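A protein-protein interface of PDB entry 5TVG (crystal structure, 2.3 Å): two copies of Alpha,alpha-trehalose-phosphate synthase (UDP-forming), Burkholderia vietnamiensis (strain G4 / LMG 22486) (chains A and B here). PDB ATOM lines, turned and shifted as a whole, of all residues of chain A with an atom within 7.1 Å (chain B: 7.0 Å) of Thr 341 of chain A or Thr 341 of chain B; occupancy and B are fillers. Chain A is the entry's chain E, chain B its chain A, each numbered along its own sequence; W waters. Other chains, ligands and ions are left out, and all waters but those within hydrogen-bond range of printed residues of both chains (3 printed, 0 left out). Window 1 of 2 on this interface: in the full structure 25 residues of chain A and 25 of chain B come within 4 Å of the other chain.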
ATOM      1  N   ARG A 265     -14.115 -17.135 -10.513  1.00  0.00           N
ATOM      2  CA  ARG A 265     -13.118 -17.832  -9.713  1.00  0.00           C
ATOM      3  C   ARG A 265     -13.150 -17.304  -8.276  1.00  0.00           C
ATOM      4  O   ARG A 265     -13.457 -16.134  -8.024  1.00  0.00           O
ATOM      5  CB  ARG A 265     -11.733 -17.652 -10.331  1.00  0.00           C
ATOM      6  CG  ARG A 265     -11.591 -18.333 -11.685  1.00  0.00           C
ATOM      7  CD  ARG A 265     -10.360 -17.844 -12.417  1.00  0.00           C
ATOM      8  NE  ARG A 265     -10.149 -18.528 -13.684  1.00  0.00           N
ATOM      9  CZ  ARG A 265      -9.378 -18.060 -14.664  1.00  0.00           C
ATOM     10  NH1 ARG A 265      -8.743 -16.901 -14.518  1.00  0.00           N
ATOM     11  NH2 ARG A 265      -9.230 -18.755 -15.791  1.00  0.00           N
ATOM     12  N   PHE A 287      -0.055 -23.360  -1.492  1.00  0.00           N
ATOM     13  CA  PHE A 287      -1.069 -23.213  -2.531  1.00  0.00           C
ATOM     14  C   PHE A 287      -0.801 -24.164  -3.704  1.00  0.00           C
ATOM     15  O   PHE A 287      -1.723 -24.800  -4.222  1.00  0.00           O
ATOM     16  CB  PHE A 287      -1.104 -21.758  -2.971  1.00  0.00           C
ATOM     17  CG  PHE A 287      -2.088 -21.463  -4.068  1.00  0.00           C
ATOM     18  CD1 PHE A 287      -3.452 -21.570  -3.850  1.00  0.00           C
ATOM     19  CD2 PHE A 287      -1.646 -21.006  -5.299  1.00  0.00           C
ATOM     20  CE1 PHE A 287      -4.353 -21.271  -4.849  1.00  0.00           C
ATOM     21  CE2 PHE A 287      -2.551 -20.689  -6.305  1.00  0.00           C
ATOM     22  CZ  PHE A 287      -3.900 -20.819  -6.077  1.00  0.00           C
ATOM     23  N   VAL A 301      -9.734 -21.101  -8.920  1.00  0.00           N
ATOM     24  CA  VAL A 301      -9.325 -20.238  -7.819  1.00  0.00           C
ATOM     25  C   VAL A 301      -8.085 -19.466  -8.250  1.00  0.00           C
ATOM     26  O   VAL A 301      -7.267 -19.952  -9.041  1.00  0.00           O
ATOM     27  CB  VAL A 301      -9.053 -21.041  -6.518  1.00  0.00           C
ATOM     28  CG1 VAL A 301      -7.978 -22.114  -6.766  1.00  0.00           C
ATOM     29  CG2 VAL A 301      -8.631 -20.109  -5.385  1.00  0.00           C
ATOM     30  N   SER A 302      -7.957 -18.243  -7.737  1.00  0.00           N
ATOM     31  CA  SER A 302      -6.806 -17.400  -8.008  1.00  0.00           C
ATOM     32  C   SER A 302      -6.248 -16.873  -6.698  1.00  0.00           C
ATOM     33  O   SER A 302      -7.005 -16.443  -5.827  1.00  0.00           O
ATOM     34  CB  SER A 302      -7.203 -16.240  -8.923  1.00  0.00           C
ATOM     35  OG  SER A 302      -7.442 -16.708 -10.240  1.00  0.00           O
ATOM     36  N   PHE A 303      -4.923 -16.918  -6.555  1.00  0.00           N
ATOM     37  CA  PHE A 303      -4.230 -16.408  -5.374  1.00  0.00           C
ATOM     38  C   PHE A 303      -3.560 -15.076  -5.721  1.00  0.00           C
ATOM     39  O   PHE A 303      -2.600 -15.047  -6.496  1.00  0.00           O
ATOM     40  CB  PHE A 303      -3.214 -17.444  -4.885  1.00  0.00           C
ATOM     41  CG  PHE A 303      -2.383 -16.992  -3.710  1.00  0.00           C
ATOM     42  CD1 PHE A 303      -2.808 -15.955  -2.883  1.00  0.00           C
ATOM     43  CD2 PHE A 303      -1.186 -17.632  -3.418  1.00  0.00           C
ATOM     44  CE1 PHE A 303      -2.048 -15.553  -1.807  1.00  0.00           C
ATOM     45  CE2 PHE A 303      -0.415 -17.230  -2.355  1.00  0.00           C
ATOM     46  CZ  PHE A 303      -0.854 -16.191  -1.533  1.00  0.00           C
ATOM     47  N   ASN A 332       3.710 -20.935 -11.212  1.00  0.00           N
ATOM     48  CA  ASN A 332       2.852 -20.536 -12.320  1.00  0.00           C
ATOM     49  C   ASN A 332       3.173 -21.334 -13.579  1.00  0.00           C
ATOM     50  O   ASN A 332       2.264 -21.770 -14.274  1.00  0.00           O
ATOM     51  CB  ASN A 332       2.953 -19.034 -12.562  1.00  0.00           C
ATOM     52  CG  ASN A 332       2.173 -18.249 -11.523  1.00  0.00           C
ATOM     53  OD1 ASN A 332       1.200 -18.759 -10.961  1.00  0.00           O
ATOM     54  ND2 ASN A 332       2.598 -17.030 -11.247  1.00  0.00           N
ATOM     55  N   PHE A 335       1.399 -24.809 -13.389  1.00  0.00           N
ATOM     56  CA  PHE A 335      -0.051 -24.964 -13.421  1.00  0.00           C
ATOM     57  C   PHE A 335      -0.776 -23.963 -14.306  1.00  0.00           C
ATOM     58  O   PHE A 335      -1.985 -24.130 -14.536  1.00  0.00           O
ATOM     59  CB  PHE A 335      -0.635 -24.835 -12.005  1.00  0.00           C
ATOM     60  CG  PHE A 335      -0.357 -26.005 -11.105  1.00  0.00           C
ATOM     61  CD1 PHE A 335      -0.774 -27.289 -11.437  1.00  0.00           C
ATOM     62  CD2 PHE A 335       0.283 -25.811  -9.886  1.00  0.00           C
ATOM     63  CE1 PHE A 335      -0.523 -28.364 -10.575  1.00  0.00           C
ATOM     64  CE2 PHE A 335       0.527 -26.868  -9.027  1.00  0.00           C
ATOM     65  CZ  PHE A 335       0.131 -28.142  -9.371  1.00  0.00           C
ATOM     66  N   ALA A 336      -0.110 -22.916 -14.779  1.00  0.00           N
ATOM     67  CA  ALA A 336      -0.861 -21.917 -15.526  1.00  0.00           C
ATOM     68  C   ALA A 336      -1.511 -22.545 -16.756  1.00  0.00           C
ATOM     69  O   ALA A 336      -0.971 -23.468 -17.377  1.00  0.00           O
ATOM     70  CB  ALA A 336       0.040 -20.764 -15.952  1.00  0.00           C
ATOM     71  N   GLN A 337      -2.686 -22.028 -17.092  1.00  0.00           N
ATOM     72  CA  GLN A 337      -3.369 -22.280 -18.348  1.00  0.00           C
ATOM     73  C   GLN A 337      -3.418 -20.956 -19.113  1.00  0.00           C
ATOM     74  O   GLN A 337      -3.104 -19.892 -18.566  1.00  0.00           O
ATOM     75  CB  GLN A 337      -4.766 -22.854 -18.086  1.00  0.00           C
ATOM     76  CG  GLN A 337      -4.719 -24.199 -17.299  1.00  0.00           C
ATOM     77  CD  GLN A 337      -6.052 -24.617 -16.700  1.00  0.00           C
ATOM     78  OE1 GLN A 337      -7.110 -24.162 -17.130  1.00  0.00           O
ATOM     79  NE2 GLN A 337      -6.004 -25.475 -15.680  1.00  0.00           N
ATOM     80  N   LEU A 338      -3.818 -21.023 -20.387  1.00  0.00           N
ATOM     81  CA  LEU A 338      -3.737 -19.853 -21.268  1.00  0.00           C
ATOM     82  C   LEU A 338      -4.616 -18.689 -20.816  1.00  0.00           C
ATOM     83  O   LEU A 338      -4.438 -17.571 -21.319  1.00  0.00           O
ATOM     84  CB  LEU A 338      -4.086 -20.278 -22.702  1.00  0.00           C
ATOM     85  CG  LEU A 338      -2.943 -21.134 -23.273  1.00  0.00           C
ATOM     86  CD1 LEU A 338      -3.409 -21.981 -24.440  1.00  0.00           C
ATOM     87  CD2 LEU A 338      -1.800 -20.221 -23.732  1.00  0.00           C
ATOM     88  N   ASP A 339      -5.562 -18.911 -19.897  1.00  0.00           N
ATOM     89  CA  ASP A 339      -6.364 -17.819 -19.340  1.00  0.00           C
ATOM     90  C   ASP A 339      -6.321 -17.818 -17.809  1.00  0.00           C
ATOM     91  O   ASP A 339      -7.294 -17.440 -17.158  1.00  0.00           O
ATOM     92  CB  ASP A 339      -7.809 -17.879 -19.840  1.00  0.00           C
ATOM     93  CG  ASP A 339      -8.550 -19.139 -19.385  1.00  0.00           C
ATOM     94  OD1 ASP A 339      -7.925 -20.042 -18.784  1.00  0.00           O
ATOM     95  OD2 ASP A 339      -9.778 -19.222 -19.626  1.00  0.00           O
ATOM     96  N   TRP A 340      -5.254 -18.342 -17.208  1.00  0.00           N
ATOM     97  CA  TRP A 340      -5.248 -18.483 -15.756  1.00  0.00           C
ATOM     98  C   TRP A 340      -3.821 -18.401 -15.235  1.00  0.00           C
ATOM     99  O   TRP A 340      -3.006 -19.299 -15.479  1.00  0.00           O
ATOM    100  CB  TRP A 340      -5.896 -19.795 -15.328  1.00  0.00           C
ATOM    101  CG  TRP A 340      -5.946 -19.985 -13.840  1.00  0.00           C
ATOM    102  CD1 TRP A 340      -6.544 -19.154 -12.927  1.00  0.00           C
ATOM    103  CD2 TRP A 340      -5.398 -21.074 -13.087  1.00  0.00           C
ATOM    104  NE1 TRP A 340      -6.403 -19.663 -11.658  1.00  0.00           N
ATOM    105  CE2 TRP A 340      -5.706 -20.840 -11.729  1.00  0.00           C
ATOM    106  CE3 TRP A 340      -4.677 -22.220 -13.425  1.00  0.00           C
ATOM    107  CZ2 TRP A 340      -5.308 -21.705 -10.714  1.00  0.00           C
ATOM    108  CZ3 TRP A 340      -4.291 -23.089 -12.410  1.00  0.00           C
ATOM    109  CH2 TRP A 340      -4.605 -22.825 -11.077  1.00  0.00           C
ATOM    110  N   THR A 341      -3.549 -17.345 -14.478  1.00  0.00           N
ATOM    111  CA  THR A 341      -2.309 -17.220 -13.731  1.00  0.00           C
ATOM    112  C   THR A 341      -2.598 -17.653 -12.301  1.00  0.00           C
ATOM    113  O   THR A 341      -3.361 -16.966 -11.605  1.00  0.00           O
ATOM    114  CB  THR A 341      -1.812 -15.772 -13.781  1.00  0.00           C
ATOM    115  OG1 THR A 341      -1.546 -15.419 -15.148  1.00  0.00           O
ATOM    116  CG2 THR A 341      -0.547 -15.605 -12.982  1.00  0.00           C
ATOM    117  N   PRO A 342      -2.049 -18.777 -11.833  1.00  0.00           N
ATOM    118  CA  PRO A 342      -2.430 -19.279 -10.499  1.00  0.00           C
ATOM    119  C   PRO A 342      -2.140 -18.307  -9.374  1.00  0.00           C
ATOM    120  O   PRO A 342      -3.022 -18.033  -8.556  1.00  0.00           O
ATOM    121  CB  PRO A 342      -1.599 -20.563 -10.366  1.00  0.00           C
ATOM    122  CG  PRO A 342      -1.376 -21.005 -11.845  1.00  0.00           C
ATOM    123  CD  PRO A 342      -1.234 -19.742 -12.593  1.00  0.00           C
ATOM    124  N   ILE A 343      -0.923 -17.783  -9.306  1.00  0.00           N
ATOM    125  CA  ILE A 343      -0.517 -16.838  -8.276  1.00  0.00           C
ATOM    126  C   ILE A 343      -0.249 -15.501  -8.965  1.00  0.00           C
ATOM    127  O   ILE A 343       0.717 -15.376  -9.722  1.00  0.00           O
ATOM    128  CB  ILE A 343       0.730 -17.322  -7.522  1.00  0.00           C
ATOM    129  CG1 ILE A 343       0.464 -18.671  -6.838  1.00  0.00           C
ATOM    130  CG2 ILE A 343       1.207 -16.217  -6.523  1.00  0.00           C
ATOM    131  CD1 ILE A 343       1.653 -19.206  -6.059  1.00  0.00           C
ATOM    132  N   GLN A 344      -1.092 -14.500  -8.721  1.00  0.00           N
ATOM    133  CA  GLN A 344      -0.846 -13.150  -9.233  1.00  0.00           C
ATOM    134  C   GLN A 344       0.026 -12.425  -8.218  1.00  0.00           C
ATOM    135  O   GLN A 344      -0.445 -11.995  -7.162  1.00  0.00           O
ATOM    136  CB  GLN A 344      -2.149 -12.397  -9.478  1.00  0.00           C
ATOM    137  CG  GLN A 344      -3.036 -13.052 -10.535  1.00  0.00           C
ATOM    138  CD  GLN A 344      -4.373 -12.361 -10.654  1.00  0.00           C
ATOM    139  OE1 GLN A 344      -4.442 -11.125 -10.779  1.00  0.00           O
ATOM    140  NE2 GLN A 344      -5.447 -13.141 -10.611  1.00  0.00           N
ATOM    141  N   TYR A 345       1.302 -12.293  -8.538  1.00  0.00           N
ATOM    142  CA  TYR A 345       2.290 -11.743  -7.628  1.00  0.00           C
ATOM    143  C   TYR A 345       2.576 -10.303  -8.053  1.00  0.00           C
ATOM    144  O   TYR A 345       2.982 -10.056  -9.198  1.00  0.00           O
ATOM    145  CB  TYR A 345       3.546 -12.623  -7.651  1.00  0.00           C
ATOM    146  CG  TYR A 345       4.773 -12.039  -6.960  1.00  0.00           C
ATOM    147  CD1 TYR A 345       4.787 -11.782  -5.581  1.00  0.00           C
ATOM    148  CD2 TYR A 345       5.918 -11.738  -7.697  1.00  0.00           C
ATOM    149  CE1 TYR A 345       5.923 -11.239  -4.968  1.00  0.00           C
ATOM    150  CE2 TYR A 345       7.039 -11.198  -7.100  1.00  0.00           C
ATOM    151  CZ  TYR A 345       7.049 -10.949  -5.743  1.00  0.00           C
ATOM    152  OH  TYR A 345       8.190 -10.401  -5.179  1.00  0.00           O
ATOM    153  N   ARG B 265      -6.048  -7.296 -26.374  1.00  0.00           N
ATOM    154  CA  ARG B 265      -4.615  -7.067 -26.228  1.00  0.00           C
ATOM    155  C   ARG B 265      -3.841  -7.740 -27.354  1.00  0.00           C
ATOM    156  O   ARG B 265      -4.240  -8.786 -27.868  1.00  0.00           O
ATOM    157  CB  ARG B 265      -4.130  -7.595 -24.888  1.00  0.00           C
ATOM    158  CG  ARG B 265      -4.673  -6.803 -23.717  1.00  0.00           C
ATOM    159  CD  ARG B 265      -4.498  -7.560 -22.424  1.00  0.00           C
ATOM    160  NE  ARG B 265      -4.933  -6.753 -21.287  1.00  0.00           N
ATOM    161  CZ  ARG B 265      -5.248  -7.261 -20.101  1.00  0.00           C
ATOM    162  NH1 ARG B 265      -5.181  -8.576 -19.907  1.00  0.00           N
ATOM    163  NH2 ARG B 265      -5.626  -6.458 -19.115  1.00  0.00           N
ATOM    164  N   PHE B 287      11.725  -8.076 -23.360  1.00  0.00           N
ATOM    165  CA  PHE B 287      10.324  -7.696 -23.262  1.00  0.00           C
ATOM    166  C   PHE B 287      10.110  -6.782 -22.056  1.00  0.00           C
ATOM    167  O   PHE B 287       9.346  -5.818 -22.121  1.00  0.00           O
ATOM    168  CB  PHE B 287       9.461  -8.949 -23.154  1.00  0.00           C
ATOM    169  CG  PHE B 287       7.983  -8.672 -23.072  1.00  0.00           C
ATOM    170  CD1 PHE B 287       7.293  -8.171 -24.168  1.00  0.00           C
ATOM    171  CD2 PHE B 287       7.285  -8.897 -21.883  1.00  0.00           C
ATOM    172  CE1 PHE B 287       5.922  -7.922 -24.097  1.00  0.00           C
ATOM    173  CE2 PHE B 287       5.923  -8.644 -21.804  1.00  0.00           C
ATOM    174  CZ  PHE B 287       5.243  -8.166 -22.903  1.00  0.00           C
ATOM    175  N   VAL B 301      -0.459  -5.456 -24.299  1.00  0.00           N
ATOM    176  CA  VAL B 301       0.173  -6.570 -24.990  1.00  0.00           C
ATOM    177  C   VAL B 301       0.529  -7.649 -23.966  1.00  0.00           C
ATOM    178  O   VAL B 301       0.824  -7.355 -22.803  1.00  0.00           O
ATOM    179  CB  VAL B 301       1.406  -6.068 -25.783  1.00  0.00           C
ATOM    180  CG1 VAL B 301       2.364  -5.347 -24.866  1.00  0.00           C
ATOM    181  CG2 VAL B 301       2.093  -7.215 -26.509  1.00  0.00           C
ATOM    182  N   SER B 302       0.476  -8.911 -24.401  1.00  0.00           N
ATOM    183  CA  SER B 302       0.832 -10.043 -23.561  1.00  0.00           C
ATOM    184  C   SER B 302       1.839 -10.933 -24.272  1.00  0.00           C
ATOM    185  O   SER B 302       1.727 -11.177 -25.476  1.00  0.00           O
ATOM    186  CB  SER B 302      -0.401 -10.873 -23.150  1.00  0.00           C
ATOM    187  OG  SER B 302      -1.168 -10.190 -22.150  1.00  0.00           O
ATOM    188  N   PHE B 303       2.838 -11.379 -23.518  1.00  0.00           N
ATOM    189  CA  PHE B 303       3.883 -12.267 -23.996  1.00  0.00           C
ATOM    190  C   PHE B 303       3.573 -13.667 -23.451  1.00  0.00           C
ATOM    191  O   PHE B 303       3.618 -13.889 -22.237  1.00  0.00           O
ATOM    192  CB  PHE B 303       5.262 -11.744 -23.562  1.00  0.00           C
ATOM    193  CG  PHE B 303       6.429 -12.644 -23.950  1.00  0.00           C
ATOM    194  CD1 PHE B 303       6.296 -13.596 -24.976  1.00  0.00           C
ATOM    195  CD2 PHE B 303       7.660 -12.517 -23.321  1.00  0.00           C
ATOM    196  CE1 PHE B 303       7.348 -14.423 -25.323  1.00  0.00           C
ATOM    197  CE2 PHE B 303       8.720 -13.318 -23.659  1.00  0.00           C
ATOM    198  CZ  PHE B 303       8.558 -14.289 -24.687  1.00  0.00           C
ATOM    199  N   ASN B 332       7.122 -10.194 -13.885  1.00  0.00           N
ATOM    200  CA  ASN B 332       5.689 -10.097 -13.604  1.00  0.00           C
ATOM    201  C   ASN B 332       5.409  -9.326 -12.310  1.00  0.00           C
ATOM    202  O   ASN B 332       4.455  -8.547 -12.239  1.00  0.00           O
ATOM    203  CB  ASN B 332       5.080 -11.502 -13.545  1.00  0.00           C
ATOM    204  CG  ASN B 332       4.914 -12.120 -14.929  1.00  0.00           C
ATOM    205  OD1 ASN B 332       4.750 -11.406 -15.918  1.00  0.00           O
ATOM    206  ND2 ASN B 332       4.968 -13.451 -15.005  1.00  0.00           N
ATOM    207  N   PHE B 335       5.650  -5.537 -13.237  1.00  0.00           N
ATOM    208  CA  PHE B 335       4.733  -4.832 -14.126  1.00  0.00           C
ATOM    209  C   PHE B 335       3.292  -5.316 -14.050  1.00  0.00           C
ATOM    210  O   PHE B 335       2.414  -4.657 -14.624  1.00  0.00           O
ATOM    211  CB  PHE B 335       5.208  -4.935 -15.593  1.00  0.00           C
ATOM    212  CG  PHE B 335       6.414  -4.097 -15.904  1.00  0.00           C
ATOM    213  CD1 PHE B 335       6.384  -2.725 -15.725  1.00  0.00           C
ATOM    214  CD2 PHE B 335       7.573  -4.680 -16.388  1.00  0.00           C
ATOM    215  CE1 PHE B 335       7.502  -1.936 -16.009  1.00  0.00           C
ATOM    216  CE2 PHE B 335       8.696  -3.902 -16.688  1.00  0.00           C
ATOM    217  CZ  PHE B 335       8.658  -2.525 -16.497  1.00  0.00           C
ATOM    218  N   ALA B 336       3.015  -6.427 -13.368  1.00  0.00           N
ATOM    219  CA  ALA B 336       1.669  -6.986 -13.412  1.00  0.00           C
ATOM    220  C   ALA B 336       0.659  -5.999 -12.859  1.00  0.00           C
ATOM    221  O   ALA B 336       0.967  -5.166 -11.998  1.00  0.00           O
ATOM    222  CB  ALA B 336       1.565  -8.317 -12.626  1.00  0.00           C
ATOM    223  N   GLN B 337      -0.547  -6.074 -13.400  1.00  0.00           N
ATOM    224  CA  GLN B 337      -1.719  -5.399 -12.863  1.00  0.00           C
ATOM    225  C   GLN B 337      -2.740  -6.468 -12.484  1.00  0.00           C
ATOM    226  O   GLN B 337      -2.589  -7.646 -12.822  1.00  0.00           O
ATOM    227  CB  GLN B 337      -2.290  -4.397 -13.886  1.00  0.00           C
ATOM    228  CG  GLN B 337      -1.294  -3.303 -14.267  1.00  0.00           C
ATOM    229  CD  GLN B 337      -1.677  -2.524 -15.530  1.00  0.00           C
ATOM    230  OE1 GLN B 337      -2.836  -2.532 -15.961  1.00  0.00           O
ATOM    231  NE2 GLN B 337      -0.692  -1.844 -16.129  1.00  0.00           N
ATOM    232  N   LEU B 338      -3.798  -6.047 -11.793  1.00  0.00           N
ATOM    233  CA  LEU B 338      -4.761  -6.993 -11.234  1.00  0.00           C
ATOM    234  C   LEU B 338      -5.483  -7.799 -12.299  1.00  0.00           C
ATOM    235  O   LEU B 338      -6.088  -8.833 -11.976  1.00  0.00           O
ATOM    236  CB  LEU B 338      -5.769  -6.236 -10.377  1.00  0.00           C
ATOM    237  CG  LEU B 338      -5.121  -5.704  -9.093  1.00  0.00           C
ATOM    238  CD1 LEU B 338      -5.996  -4.654  -8.450  1.00  0.00           C
ATOM    239  CD2 LEU B 338      -4.829  -6.846  -8.119  1.00  0.00           C
ATOM    240  N   ASP B 339      -5.429  -7.367 -13.565  1.00  0.00           N
ATOM    241  CA  ASP B 339      -6.033  -8.138 -14.645  1.00  0.00           C
ATOM    242  C   ASP B 339      -5.050  -8.388 -15.780  1.00  0.00           C
ATOM    243  O   ASP B 339      -5.469  -8.638 -16.913  1.00  0.00           O
ATOM    244  CB  ASP B 339      -7.293  -7.459 -15.183  1.00  0.00           C
ATOM    245  CG  ASP B 339      -7.003  -6.129 -15.850  1.00  0.00           C
ATOM    246  OD1 ASP B 339      -5.852  -5.667 -15.800  1.00  0.00           O
ATOM    247  OD2 ASP B 339      -7.939  -5.546 -16.421  1.00  0.00           O
ATOM    248  N   TRP B 340      -3.754  -8.347 -15.501  1.00  0.00           N
ATOM    249  CA  TRP B 340      -2.768  -8.451 -16.568  1.00  0.00           C
ATOM    250  C   TRP B 340      -1.504  -9.104 -16.041  1.00  0.00           C
ATOM    251  O   TRP B 340      -0.801  -8.509 -15.220  1.00  0.00           O
ATOM    252  CB  TRP B 340      -2.439  -7.072 -17.140  1.00  0.00           C
ATOM    253  CG  TRP B 340      -1.431  -7.123 -18.228  1.00  0.00           C
ATOM    254  CD1 TRP B 340      -1.514  -7.849 -19.379  1.00  0.00           C
ATOM    255  CD2 TRP B 340      -0.197  -6.395 -18.299  1.00  0.00           C
ATOM    256  NE1 TRP B 340      -0.399  -7.630 -20.165  1.00  0.00           N
ATOM    257  CE2 TRP B 340       0.422  -6.739 -19.526  1.00  0.00           C
ATOM    258  CE3 TRP B 340       0.447  -5.484 -17.446  1.00  0.00           C
ATOM    259  CZ2 TRP B 340       1.658  -6.209 -19.924  1.00  0.00           C
ATOM    260  CZ3 TRP B 340       1.687  -4.957 -17.841  1.00  0.00           C
ATOM    261  CH2 TRP B 340       2.271  -5.315 -19.080  1.00  0.00           C
ATOM    262  N   THR B 341      -1.198 -10.299 -16.563  1.00  0.00           N
ATOM    263  CA  THR B 341       0.077 -10.959 -16.336  1.00  0.00           C
ATOM    264  C   THR B 341       0.965 -10.642 -17.540  1.00  0.00           C
ATOM    265  O   THR B 341       0.652 -11.089 -18.658  1.00  0.00           O
ATOM    266  CB  THR B 341      -0.115 -12.472 -16.205  1.00  0.00           C
ATOM    267  OG1 THR B 341      -0.976 -12.771 -15.102  1.00  0.00           O
ATOM    268  CG2 THR B 341       1.219 -13.173 -16.014  1.00  0.00           C
ATOM    269  N   PRO B 342       2.063  -9.898 -17.380  1.00  0.00           N
ATOM    270  CA  PRO B 342       2.869  -9.528 -18.562  1.00  0.00           C
ATOM    271  C   PRO B 342       3.401 -10.713 -19.347  1.00  0.00           C
ATOM    272  O   PRO B 342       3.262 -10.742 -20.583  1.00  0.00           O
ATOM    273  CB  PRO B 342       3.998  -8.691 -17.959  1.00  0.00           C
ATOM    274  CG  PRO B 342       3.358  -8.085 -16.683  1.00  0.00           C
ATOM    275  CD  PRO B 342       2.470  -9.163 -16.164  1.00  0.00           C
ATOM    276  N   ILE B 343       4.026 -11.676 -18.665  1.00  0.00           N
ATOM    277  CA  ILE B 343       4.607 -12.864 -19.276  1.00  0.00           C
ATOM    278  C   ILE B 343       3.839 -14.079 -18.762  1.00  0.00           C
ATOM    279  O   ILE B 343       3.949 -14.441 -17.580  1.00  0.00           O
ATOM    280  CB  ILE B 343       6.103 -12.981 -18.967  1.00  0.00           C
ATOM    281  CG1 ILE B 343       6.826 -11.738 -19.482  1.00  0.00           C
ATOM    282  CG2 ILE B 343       6.705 -14.236 -19.648  1.00  0.00           C
ATOM    283  CD1 ILE B 343       8.313 -11.790 -19.291  1.00  0.00           C
ATOM    284  N   GLN B 344       3.048 -14.694 -19.638  1.00  0.00           N
ATOM    285  CA  GLN B 344       2.347 -15.941 -19.329  1.00  0.00           C
ATOM    286  C   GLN B 344       3.309 -17.064 -19.676  1.00  0.00           C
ATOM    287  O   GLN B 344       3.511 -17.394 -20.852  1.00  0.00           O
ATOM    288  CB  GLN B 344       1.040 -16.064 -20.101  1.00  0.00           C
ATOM    289  CG  GLN B 344       0.003 -14.997 -19.774  1.00  0.00           C
ATOM    290  CD  GLN B 344      -1.196 -15.058 -20.707  1.00  0.00           C
ATOM    291  OE1 GLN B 344      -1.786 -16.128 -20.917  1.00  0.00           O
ATOM    292  NE2 GLN B 344      -1.542 -13.922 -21.306  1.00  0.00           N
ATOM    293  N   TYR B 345       3.903 -17.647 -18.643  1.00  0.00           N
ATOM    294  CA  TYR B 345       4.951 -18.646 -18.777  1.00  0.00           C
ATOM    295  C   TYR B 345       4.364 -20.026 -18.496  1.00  0.00           C
ATOM    296  O   TYR B 345       3.923 -20.298 -17.376  1.00  0.00           O
ATOM    297  CB  TYR B 345       6.098 -18.293 -17.827  1.00  0.00           C
ATOM    298  CG  TYR B 345       7.107 -19.380 -17.610  1.00  0.00           C
ATOM    299  CD1 TYR B 345       7.861 -19.879 -18.672  1.00  0.00           C
ATOM    300  CD2 TYR B 345       7.336 -19.895 -16.333  1.00  0.00           C
ATOM    301  CE1 TYR B 345       8.795 -20.894 -18.470  1.00  0.00           C
ATOM    302  CE2 TYR B 345       8.281 -20.891 -16.125  1.00  0.00           C
ATOM    303  CZ  TYR B 345       9.000 -21.386 -17.189  1.00  0.00           C
ATOM    304  OH  TYR B 345       9.922 -22.384 -16.966  1.00  0.00           O
HETATM  305  O   HOH W   1       5.046 -15.538 -12.660  1.00  0.00           O
HETATM  306  O   HOH W   2      -1.456 -17.543 -18.451  1.00  0.00           O
HETATM  307  O   HOH W   3      -2.060 -10.486 -12.102  1.00  0.00           O
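O of Leu 338 of chain B lies close to OE1 of Gln 344 of chain A (3.1 Å). The side-chain hydroxyl (OG1) of Thr 341 of chain B is in hydrogen-bond range of the side-chain hydroxyl (OG1) of Thr 341 of chain A (2.7 Å). The side-chain amide oxygen (OE1) of Gln 344 of chain B lies close to the backbone carbonyl oxygen (O) of Leu 338 of chain A (3.0 Å).
O of Phe 303 of chain B sits at hydrogen-bond distance from N of Gln 344 of chain B (2.8 Å). N of Ile 343 of chain B sits at hydrogen-bond distance from OD1 of Asn 332 of chain B, at 2.9 Å. N of Gln 344 of chain A is in hydrogen-bond range of O of Phe 303 of chain A (2.7 Å). OD1 of Asn 332 of chain A sits at hydrogen-bond distance from N of Ile 343 of chain A (2.9 Å).
Among the printed residues, merely in contact across the chains: Asn 332 of chain A with Tyr 345 of chain B (3.8 Å) and Tyr 345 of chain A with Asn 332 of chain B (3.7 Å).
Of chain B, only Thr 341 comes within 4 Å of Thr 341 of chain A. Thr 341 of chain B touches just one residue of chain A: Thr 341 (2.7 Å). Of the printed residues of chain A, Leu 338 of chain B touches Gln 344 (3.1 Å). Of the printed residues of chain B, Asn 332 of chain A touches Tyr 345. The nearest residue of chain A that does not touch Thr 341 of chain B is Gln 344 of chain A (5.0 Å). The nearest printed residue of chain A that does not touch Gln 344 of chain B is Gln 337 of chain A (4.6 Å).
Of the 17 printed residues of chain A, 5 touch a printed residue of chain B. Of the 17 printed residues of chain B, 5 touch a printed residue of chain A. Printed residues of chain B that touch a printed residue of chain A: Asn 332, Leu 338, Thr 341, Gln 344 and Tyr 345. Among the printed residues, no Asp or Glu carboxylate lies within 4 Å of a Lys or Arg side-chain nitrogen of the other chain.
Asn 332 of chain A touches Tyr 345 of chain B, and with the chains exchanged Tyr 345 of chain A touches Asn 332 of chain B. Leu 338 of chain A touches Gln 344 of chain B, and with the chains exchanged Gln 344 of chain A touches Leu 338 of chain B. Thr 341 of chain B touches its own counterpart, Thr 341 of chain A. 17 positions are printed for both chains. Of the 5 pairs that touch across the chains among the printed residues, 5 have their exchanged pair printed and touching as well.
Water W3 bridges the side-chain amide oxygen of Gln 344 of chain A and the backbone carbonyl oxygen of Gln 337 of chain B. Water W2 lies within hydrogen-bond range of OE1 of Gln 344 of chain B and O of Gln 337 of chain A. Water W1 lies within hydrogen-bond range of ND2 of Asn 332 of chain B (3.1 Å) and ND2 of Asn 332 of chain A (3.2 Å).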
